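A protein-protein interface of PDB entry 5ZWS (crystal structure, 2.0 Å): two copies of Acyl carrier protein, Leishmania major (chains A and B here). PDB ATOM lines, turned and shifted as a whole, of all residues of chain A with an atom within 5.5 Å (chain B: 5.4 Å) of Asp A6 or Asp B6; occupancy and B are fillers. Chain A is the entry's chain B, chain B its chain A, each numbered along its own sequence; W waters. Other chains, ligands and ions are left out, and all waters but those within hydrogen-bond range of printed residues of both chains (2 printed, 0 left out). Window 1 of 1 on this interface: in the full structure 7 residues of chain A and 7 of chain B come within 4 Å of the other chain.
Water W1 lies within hydrogen-bond range of the side-chain carboxylate (OD1) of Asp A6 (2.7 Å), a ring nitrogen (ND1) of His A3 (3.0 Å) and a ring nitrogen (ND1) of His B3 (3.4 Å).
Water W2 lies within hydrogen-bond range of the side-chain carboxylate of Asp B6 and the backbone carbonyl oxygen of Asp A6.
Of the 11 printed residues of chain B, 4 touch a printed residue of chain A.
Of the 11 printed residues of chain A, 4 touch a printed residue of chain B.
Along chain A the printed residues that touch a printed residue of chain B span positions 2 to 10.
Ser A2 touches Arg B10, and with the chains exchanged Arg A10 touches Ser B2.
His A3 touches Arg B10, and with the chains exchanged Arg A10 touches His B3.
Asp B6 touches its own counterpart, Asp A6.
Asp A6 touches Arg B10, and with the chains exchanged Arg A10 touches Asp B6.
Positions printed for both chains: 2, 3, 4, 5, 6, 7, 8, 9, 10, 11 and 54.
Of the 7 pairs that touch across the chains among the printed residues, 7 have their exchanged pair printed and touching as well.
NH1 of Arg B10 is in salt-bridge range of OD1 of Asp A6, 2.9 Å away.
OD2 of Asp B6 is in salt-bridge range of NH1 of Arg A10.
Asp A6 touches just these residues of chain B: Asp B6 and Arg B10.
Leu A8 touches none of the printed residues of chain B.
Of the printed residues of chain B, Arg A10 touches Ser B2 (3.5 Å), His B3 (3.6 Å) and Asp B6 (2.9 Å).
Printed residues of chain A within 4 Å of Ser B2: Arg A10.
Of chain A, only Asp A6 (3.5 Å) and Arg A10 (2.9 Å) come within 4 Å of Asp B6.
Of the printed residues of chain A, Arg B10 touches Ser A2, His A3 and Asp A6.
Val B11 touches none of the printed residues of chain A.
The nearest residue of chain B that does not touch Asp A6 is Val B7 (5.0 Å).
The nearest printed residue of chain A that does not touch His B3 is His A3 (4.7 Å).
OG of Ser A2 is in hydrogen-bond range of N of Asn A5, 3.1 Å away.
The side-chain hydroxyl of Ser B2 lies within hydrogen-bond range of the backbone NH of Asn B5.
Among the printed residues, merely in contact across the chains: Arg A10 with Ser B2, Asp A6 with Asp B6, Arg A10 with His B3, Ser A2 with Arg B10 and His A3 with Arg B10.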
ATOM      1  N   SER A   2       0.335 -23.854 -32.933  1.00  0.00           N
ATOM      2  CA  SER A   2       0.595 -25.150 -33.546  1.00  0.00           C
ATOM      3  C   SER A   2       1.791 -25.779 -32.851  1.00  0.00           C
ATOM      4  O   SER A   2       2.568 -25.098 -32.176  1.00  0.00           O
ATOM      5  CB  SER A   2       0.850 -25.029 -35.054  1.00  0.00           C
ATOM      6  OG  SER A   2       2.073 -24.364 -35.322  1.00  0.00           O
ATOM      7  N   HIS A   3       1.921 -27.097 -33.019  1.00  0.00           N
ATOM      8  CA  HIS A   3       3.055 -27.806 -32.434  1.00  0.00           C
ATOM      9  C   HIS A   3       4.368 -27.318 -33.029  1.00  0.00           C
ATOM     10  O   HIS A   3       5.360 -27.149 -32.311  1.00  0.00           O
ATOM     11  CB  HIS A   3       2.892 -29.313 -32.641  1.00  0.00           C
ATOM     12  CG  HIS A   3       4.022 -30.124 -32.087  1.00  0.00           C
ATOM     13  ND1 HIS A   3       4.345 -30.131 -30.748  1.00  0.00           N
ATOM     14  CD2 HIS A   3       4.899 -30.961 -32.690  1.00  0.00           C
ATOM     15  CE1 HIS A   3       5.375 -30.935 -30.549  1.00  0.00           C
ATOM     16  NE2 HIS A   3       5.731 -31.451 -31.714  1.00  0.00           N
ATOM     17  N   MET A   4       4.390 -27.078 -34.343  1.00  0.00           N
ATOM     18  CA  MET A   4       5.583 -26.532 -34.979  1.00  0.00           C
ATOM     19  C   MET A   4       5.923 -25.160 -34.410  1.00  0.00           C
ATOM     20  O   MET A   4       7.099 -24.849 -34.184  1.00  0.00           O
ATOM     21  CB  MET A   4       5.373 -26.473 -36.497  1.00  0.00           C
ATOM     22  CG  MET A   4       6.537 -25.917 -37.314  1.00  0.00           C
ATOM     23  SD  MET A   4       6.678 -24.116 -37.288  1.00  0.00           S
ATOM     24  CE  MET A   4       5.542 -23.674 -38.603  1.00  0.00           C
ATOM     25  N   ASN A   5       4.907 -24.328 -34.167  1.00  0.00           N
ATOM     26  CA  ASN A   5       5.155 -23.018 -33.576  1.00  0.00           C
ATOM     27  C   ASN A   5       5.603 -23.141 -32.124  1.00  0.00           C
ATOM     28  O   ASN A   5       6.441 -22.357 -31.659  1.00  0.00           O
ATOM     29  CB  ASN A   5       3.904 -22.148 -33.685  1.00  0.00           C
ATOM     30  CG  ASN A   5       4.163 -20.709 -33.306  1.00  0.00           C
ATOM     31  OD1 ASN A   5       3.590 -20.192 -32.349  1.00  0.00           O
ATOM     32  ND2 ASN A   5       5.042 -20.053 -34.053  1.00  0.00           N
ATOM     33  N   ASP A   6       5.044 -24.109 -31.390  1.00  0.00           N
ATOM     34  CA  ASP A   6       5.524 -24.383 -30.039  1.00  0.00           C
ATOM     35  C   ASP A   6       7.006 -24.750 -30.053  1.00  0.00           C
ATOM     36  O   ASP A   6       7.782 -24.284 -29.210  1.00  0.00           O
ATOM     37  CB  ASP A   6       4.705 -25.508 -29.404  1.00  0.00           C
ATOM     38  CG  ASP A   6       3.261 -25.116 -29.149  1.00  0.00           C
ATOM     39  OD1 ASP A   6       2.412 -26.027 -29.030  1.00  0.00           O
ATOM     40  OD2 ASP A   6       2.972 -23.904 -29.070  1.00  0.00           O
ATOM     41  N   VAL A   7       7.414 -25.583 -31.011  1.00  0.00           N
ATOM     42  CA  VAL A   7       8.821 -25.941 -31.152  1.00  0.00           C
ATOM     43  C   VAL A   7       9.642 -24.727 -31.570  1.00  0.00           C
ATOM     44  O   VAL A   7      10.672 -24.421 -30.963  1.00  0.00           O
ATOM     45  CB  VAL A   7       8.973 -27.105 -32.148  1.00  0.00           C
ATOM     46  CG1 VAL A   7      10.437 -27.328 -32.503  1.00  0.00           C
ATOM     47  CG2 VAL A   7       8.360 -28.377 -31.576  1.00  0.00           C
ATOM     48  N   LEU A   8       9.206 -24.027 -32.621  1.00  0.00           N
ATOM     49  CA  LEU A   8       9.929 -22.852 -33.104  1.00  0.00           C
ATOM     50  C   LEU A   8      10.148 -21.829 -31.996  1.00  0.00           C
ATOM     51  O   LEU A   8      11.222 -21.224 -31.904  1.00  0.00           O
ATOM     52  CB  LEU A   8       9.169 -22.215 -34.269  1.00  0.00           C
ATOM     53  CG  LEU A   8       9.580 -20.806 -34.722  1.00  0.00           C
ATOM     54  CD1 LEU A   8      11.012 -20.780 -35.233  1.00  0.00           C
ATOM     55  CD2 LEU A   8       8.626 -20.265 -35.765  1.00  0.00           C
ATOM     56  N   THR A   9       9.137 -21.622 -31.146  1.00  0.00           N
ATOM     57  CA  THR A   9       9.264 -20.647 -30.068  1.00  0.00           C
ATOM     58  C   THR A   9      10.374 -21.040 -29.101  1.00  0.00           C
ATOM     59  O   THR A   9      11.172 -20.193 -28.683  1.00  0.00           O
ATOM     60  CB  THR A   9       7.930 -20.510 -29.330  1.00  0.00           C
ATOM     61  OG1 THR A   9       6.937 -19.994 -30.225  1.00  0.00           O
ATOM     62  CG2 THR A   9       8.067 -19.561 -28.148  1.00  0.00           C
ATOM     63  N   ARG A  10      10.458 -22.326 -28.757  1.00  0.00           N
ATOM     64  CA  ARG A  10      11.471 -22.770 -27.808  1.00  0.00           C
ATOM     65  C   ARG A  10      12.856 -22.799 -28.446  1.00  0.00           C
ATOM     66  O   ARG A  10      13.852 -22.473 -27.790  1.00  0.00           O
ATOM     67  CB  ARG A  10      11.092 -24.143 -27.248  1.00  0.00           C
ATOM     68  CG  ARG A  10       9.880 -24.097 -26.323  1.00  0.00           C
ATOM     69  CD  ARG A  10       9.177 -25.444 -26.210  1.00  0.00           C
ATOM     70  NE  ARG A  10       9.957 -26.411 -25.442  1.00  0.00           N
ATOM     71  CZ  ARG A  10       9.585 -27.669 -25.225  1.00  0.00           C
ATOM     72  NH1 ARG A  10       8.438 -28.120 -25.717  1.00  0.00           N
ATOM     73  NH2 ARG A  10      10.359 -28.477 -24.512  1.00  0.00           N
ATOM     74  N   VAL A  11      12.941 -23.172 -29.725  1.00  0.00           N
ATOM     75  CA  VAL A  11      14.232 -23.173 -30.411  1.00  0.00           C
ATOM     76  C   VAL A  11      14.781 -21.756 -30.525  1.00  0.00           C
ATOM     77  O   VAL A  11      15.979 -21.519 -30.319  1.00  0.00           O
ATOM     78  CB  VAL A  11      14.105 -23.846 -31.792  1.00  0.00           C
ATOM     79  CG1 VAL A  11      15.381 -23.658 -32.598  1.00  0.00           C
ATOM     80  CG2 VAL A  11      13.782 -25.331 -31.638  1.00  0.00           C
ATOM     81  N   PHE A  54      14.272 -30.105 -25.241  1.00  0.00           N
ATOM     82  CA  PHE A  54      13.257 -31.111 -25.521  1.00  0.00           C
ATOM     83  C   PHE A  54      13.568 -32.459 -24.879  1.00  0.00           C
ATOM     84  O   PHE A  54      12.903 -33.450 -25.200  1.00  0.00           O
ATOM     85  CB  PHE A  54      13.082 -31.264 -27.036  1.00  0.00           C
ATOM     86  CG  PHE A  54      12.720 -29.978 -27.729  1.00  0.00           C
ATOM     87  CD1 PHE A  54      11.397 -29.571 -27.823  1.00  0.00           C
ATOM     88  CD2 PHE A  54      13.702 -29.169 -28.277  1.00  0.00           C
ATOM     89  CE1 PHE A  54      11.061 -28.382 -28.456  1.00  0.00           C
ATOM     90  CE2 PHE A  54      13.375 -27.981 -28.910  1.00  0.00           C
ATOM     91  CZ  PHE A  54      12.049 -27.588 -29.000  1.00  0.00           C
ATOM     92  N   SER B   2       8.203 -26.374 -22.050  1.00  0.00           N
ATOM     93  CA  SER B   2       7.802 -27.767 -21.925  1.00  0.00           C
ATOM     94  C   SER B   2       6.553 -27.983 -22.761  1.00  0.00           C
ATOM     95  O   SER B   2       5.841 -27.036 -23.099  1.00  0.00           O
ATOM     96  CB  SER B   2       7.538 -28.150 -20.466  1.00  0.00           C
ATOM     97  OG  SER B   2       6.388 -27.489 -19.965  1.00  0.00           O
ATOM     98  N   HIS B   3       6.295 -29.253 -23.085  1.00  0.00           N
ATOM     99  CA  HIS B   3       5.096 -29.578 -23.849  1.00  0.00           C
ATOM    100  C   HIS B   3       3.833 -29.247 -23.067  1.00  0.00           C
ATOM    101  O   HIS B   3       2.858 -28.745 -23.639  1.00  0.00           O
ATOM    102  CB  HIS B   3       5.092 -31.051 -24.250  1.00  0.00           C
ATOM    103  CG  HIS B   3       3.863 -31.453 -25.001  1.00  0.00           C
ATOM    104  ND1 HIS B   3       3.527 -30.907 -26.222  1.00  0.00           N
ATOM    105  CD2 HIS B   3       2.869 -32.316 -24.688  1.00  0.00           C
ATOM    106  CE1 HIS B   3       2.390 -31.435 -26.639  1.00  0.00           C
ATOM    107  NE2 HIS B   3       1.968 -32.292 -25.725  1.00  0.00           N
ATOM    108  N   MET B   4       3.827 -29.529 -21.760  1.00  0.00           N
ATOM    109  CA  MET B   4       2.668 -29.181 -20.944  1.00  0.00           C
ATOM    110  C   MET B   4       2.431 -27.677 -20.955  1.00  0.00           C
ATOM    111  O   MET B   4       1.284 -27.223 -21.028  1.00  0.00           O
ATOM    112  CB  MET B   4       2.849 -29.690 -19.509  1.00  0.00           C
ATOM    113  CG  MET B   4       1.659 -29.428 -18.570  1.00  0.00           C
ATOM    114  SD  MET B   4       1.455 -27.745 -17.920  1.00  0.00           S
ATOM    115  CE  MET B   4       2.508 -27.799 -16.478  1.00  0.00           C
ATOM    116  N   ASN B   5       3.507 -26.888 -20.887  1.00  0.00           N
ATOM    117  CA  ASN B   5       3.355 -25.439 -20.945  1.00  0.00           C
ATOM    118  C   ASN B   5       2.911 -24.989 -22.331  1.00  0.00           C
ATOM    119  O   ASN B   5       2.142 -24.030 -22.461  1.00  0.00           O
ATOM    120  CB  ASN B   5       4.662 -24.756 -20.544  1.00  0.00           C
ATOM    121  CG  ASN B   5       4.500 -23.265 -20.334  1.00  0.00           C
ATOM    122  OD1 ASN B   5       5.101 -22.455 -21.041  1.00  0.00           O
ATOM    123  ND2 ASN B   5       3.681 -22.895 -19.354  1.00  0.00           N
ATOM    124  N   ASP B   6       3.394 -25.665 -23.380  1.00  0.00           N
ATOM    125  CA  ASP B   6       2.918 -25.386 -24.733  1.00  0.00           C
ATOM    126  C   ASP B   6       1.412 -25.595 -24.843  1.00  0.00           C
ATOM    127  O   ASP B   6       0.707 -24.787 -25.458  1.00  0.00           O
ATOM    128  CB  ASP B   6       3.643 -26.278 -25.741  1.00  0.00           C
ATOM    129  CG  ASP B   6       5.124 -25.977 -25.834  1.00  0.00           C
ATOM    130  OD1 ASP B   6       5.535 -24.863 -25.451  1.00  0.00           O
ATOM    131  OD2 ASP B   6       5.876 -26.864 -26.299  1.00  0.00           O
ATOM    132  N   VAL B   7       0.906 -26.685 -24.263  1.00  0.00           N
ATOM    133  CA  VAL B   7      -0.532 -26.941 -24.269  1.00  0.00           C
ATOM    134  C   VAL B   7      -1.266 -25.915 -23.412  1.00  0.00           C
ATOM    135  O   VAL B   7      -2.229 -25.282 -23.861  1.00  0.00           O
ATOM    136  CB  VAL B   7      -0.816 -28.378 -23.800  1.00  0.00           C
ATOM    137  CG1 VAL B   7      -2.301 -28.575 -23.555  1.00  0.00           C
ATOM    138  CG2 VAL B   7      -0.302 -29.379 -24.828  1.00  0.00           C
ATOM    139  N   LEU B   8      -0.823 -25.743 -22.160  1.00  0.00           N
ATOM    140  CA  LEU B   8      -1.458 -24.790 -21.253  1.00  0.00           C
ATOM    141  C   LEU B   8      -1.510 -23.388 -21.849  1.00  0.00           C
ATOM    142  O   LEU B   8      -2.512 -22.681 -21.698  1.00  0.00           O
ATOM    143  CB  LEU B   8      -0.715 -24.765 -19.914  1.00  0.00           C
ATOM    144  CG  LEU B   8      -1.098 -23.620 -18.970  1.00  0.00           C
ATOM    145  CD1 LEU B   8      -2.566 -23.729 -18.566  1.00  0.00           C
ATOM    146  CD2 LEU B   8      -0.195 -23.557 -17.744  1.00  0.00           C
ATOM    147  N   THR B   9      -0.436 -22.968 -22.525  1.00  0.00           N
ATOM    148  CA  THR B   9      -0.403 -21.627 -23.101  1.00  0.00           C
ATOM    149  C   THR B   9      -1.495 -21.448 -24.150  1.00  0.00           C
ATOM    150  O   THR B   9      -2.170 -20.411 -24.182  1.00  0.00           O
ATOM    151  CB  THR B   9       0.974 -21.347 -23.704  1.00  0.00           C
ATOM    152  OG1 THR B   9       1.956 -21.346 -22.662  1.00  0.00           O
ATOM    153  CG2 THR B   9       0.996 -19.991 -24.405  1.00  0.00           C
ATOM    154  N   ARG B  10      -1.700 -22.458 -24.998  1.00  0.00           N
ATOM    155  CA  ARG B  10      -2.702 -22.345 -26.054  1.00  0.00           C
ATOM    156  C   ARG B  10      -4.115 -22.455 -25.490  1.00  0.00           C
ATOM    157  O   ARG B  10      -5.026 -21.759 -25.952  1.00  0.00           O
ATOM    158  CB  ARG B  10      -2.443 -23.409 -27.123  1.00  0.00           C
ATOM    159  CG  ARG B  10      -1.186 -23.142 -27.957  1.00  0.00           C
ATOM    160  CD  ARG B  10      -0.630 -24.414 -28.575  1.00  0.00           C
ATOM    161  NE  ARG B  10      -1.477 -24.935 -29.644  1.00  0.00           N
ATOM    162  CZ  ARG B  10      -1.233 -26.062 -30.304  1.00  0.00           C
ATOM    163  NH1 ARG B  10      -0.165 -26.791 -30.007  1.00  0.00           N
ATOM    164  NH2 ARG B  10      -2.058 -26.465 -31.263  1.00  0.00           N
ATOM    165  N   VAL B  11      -4.315 -23.308 -24.482  1.00  0.00           N
ATOM    166  CA  VAL B  11      -5.628 -23.417 -23.847  1.00  0.00           C
ATOM    167  C   VAL B  11      -5.993 -22.106 -23.162  1.00  0.00           C
ATOM    168  O   VAL B  11      -7.147 -21.661 -23.212  1.00  0.00           O
ATOM    169  CB  VAL B  11      -5.653 -24.598 -22.857  1.00  0.00           C
ATOM    170  CG1 VAL B  11      -6.942 -24.584 -22.041  1.00  0.00           C
ATOM    171  CG2 VAL B  11      -5.496 -25.926 -23.594  1.00  0.00           C
ATOM    172  N   PHE B  54      -6.273 -27.832 -31.173  1.00  0.00           N
ATOM    173  CA  PHE B  54      -5.389 -28.984 -31.285  1.00  0.00           C
ATOM    174  C   PHE B  54      -5.856 -29.977 -32.340  1.00  0.00           C
ATOM    175  O   PHE B  54      -5.308 -31.083 -32.420  1.00  0.00           O
ATOM    176  CB  PHE B  54      -5.253 -29.675 -29.925  1.00  0.00           C
ATOM    177  CG  PHE B  54      -4.733 -28.775 -28.841  1.00  0.00           C
ATOM    178  CD1 PHE B  54      -3.370 -28.612 -28.651  1.00  0.00           C
ATOM    179  CD2 PHE B  54      -5.607 -28.083 -28.015  1.00  0.00           C
ATOM    180  CE1 PHE B  54      -2.887 -27.784 -27.656  1.00  0.00           C
ATOM    181  CE2 PHE B  54      -5.131 -27.252 -27.020  1.00  0.00           C
ATOM    182  CZ  PHE B  54      -3.768 -27.103 -26.839  1.00  0.00           C
HETATM  183  O   HOH W   1       2.816 -28.631 -28.712  1.00  0.00           O
HETATM  184  O   HOH W   2       6.642 -22.853 -26.987  1.00  0.00           O
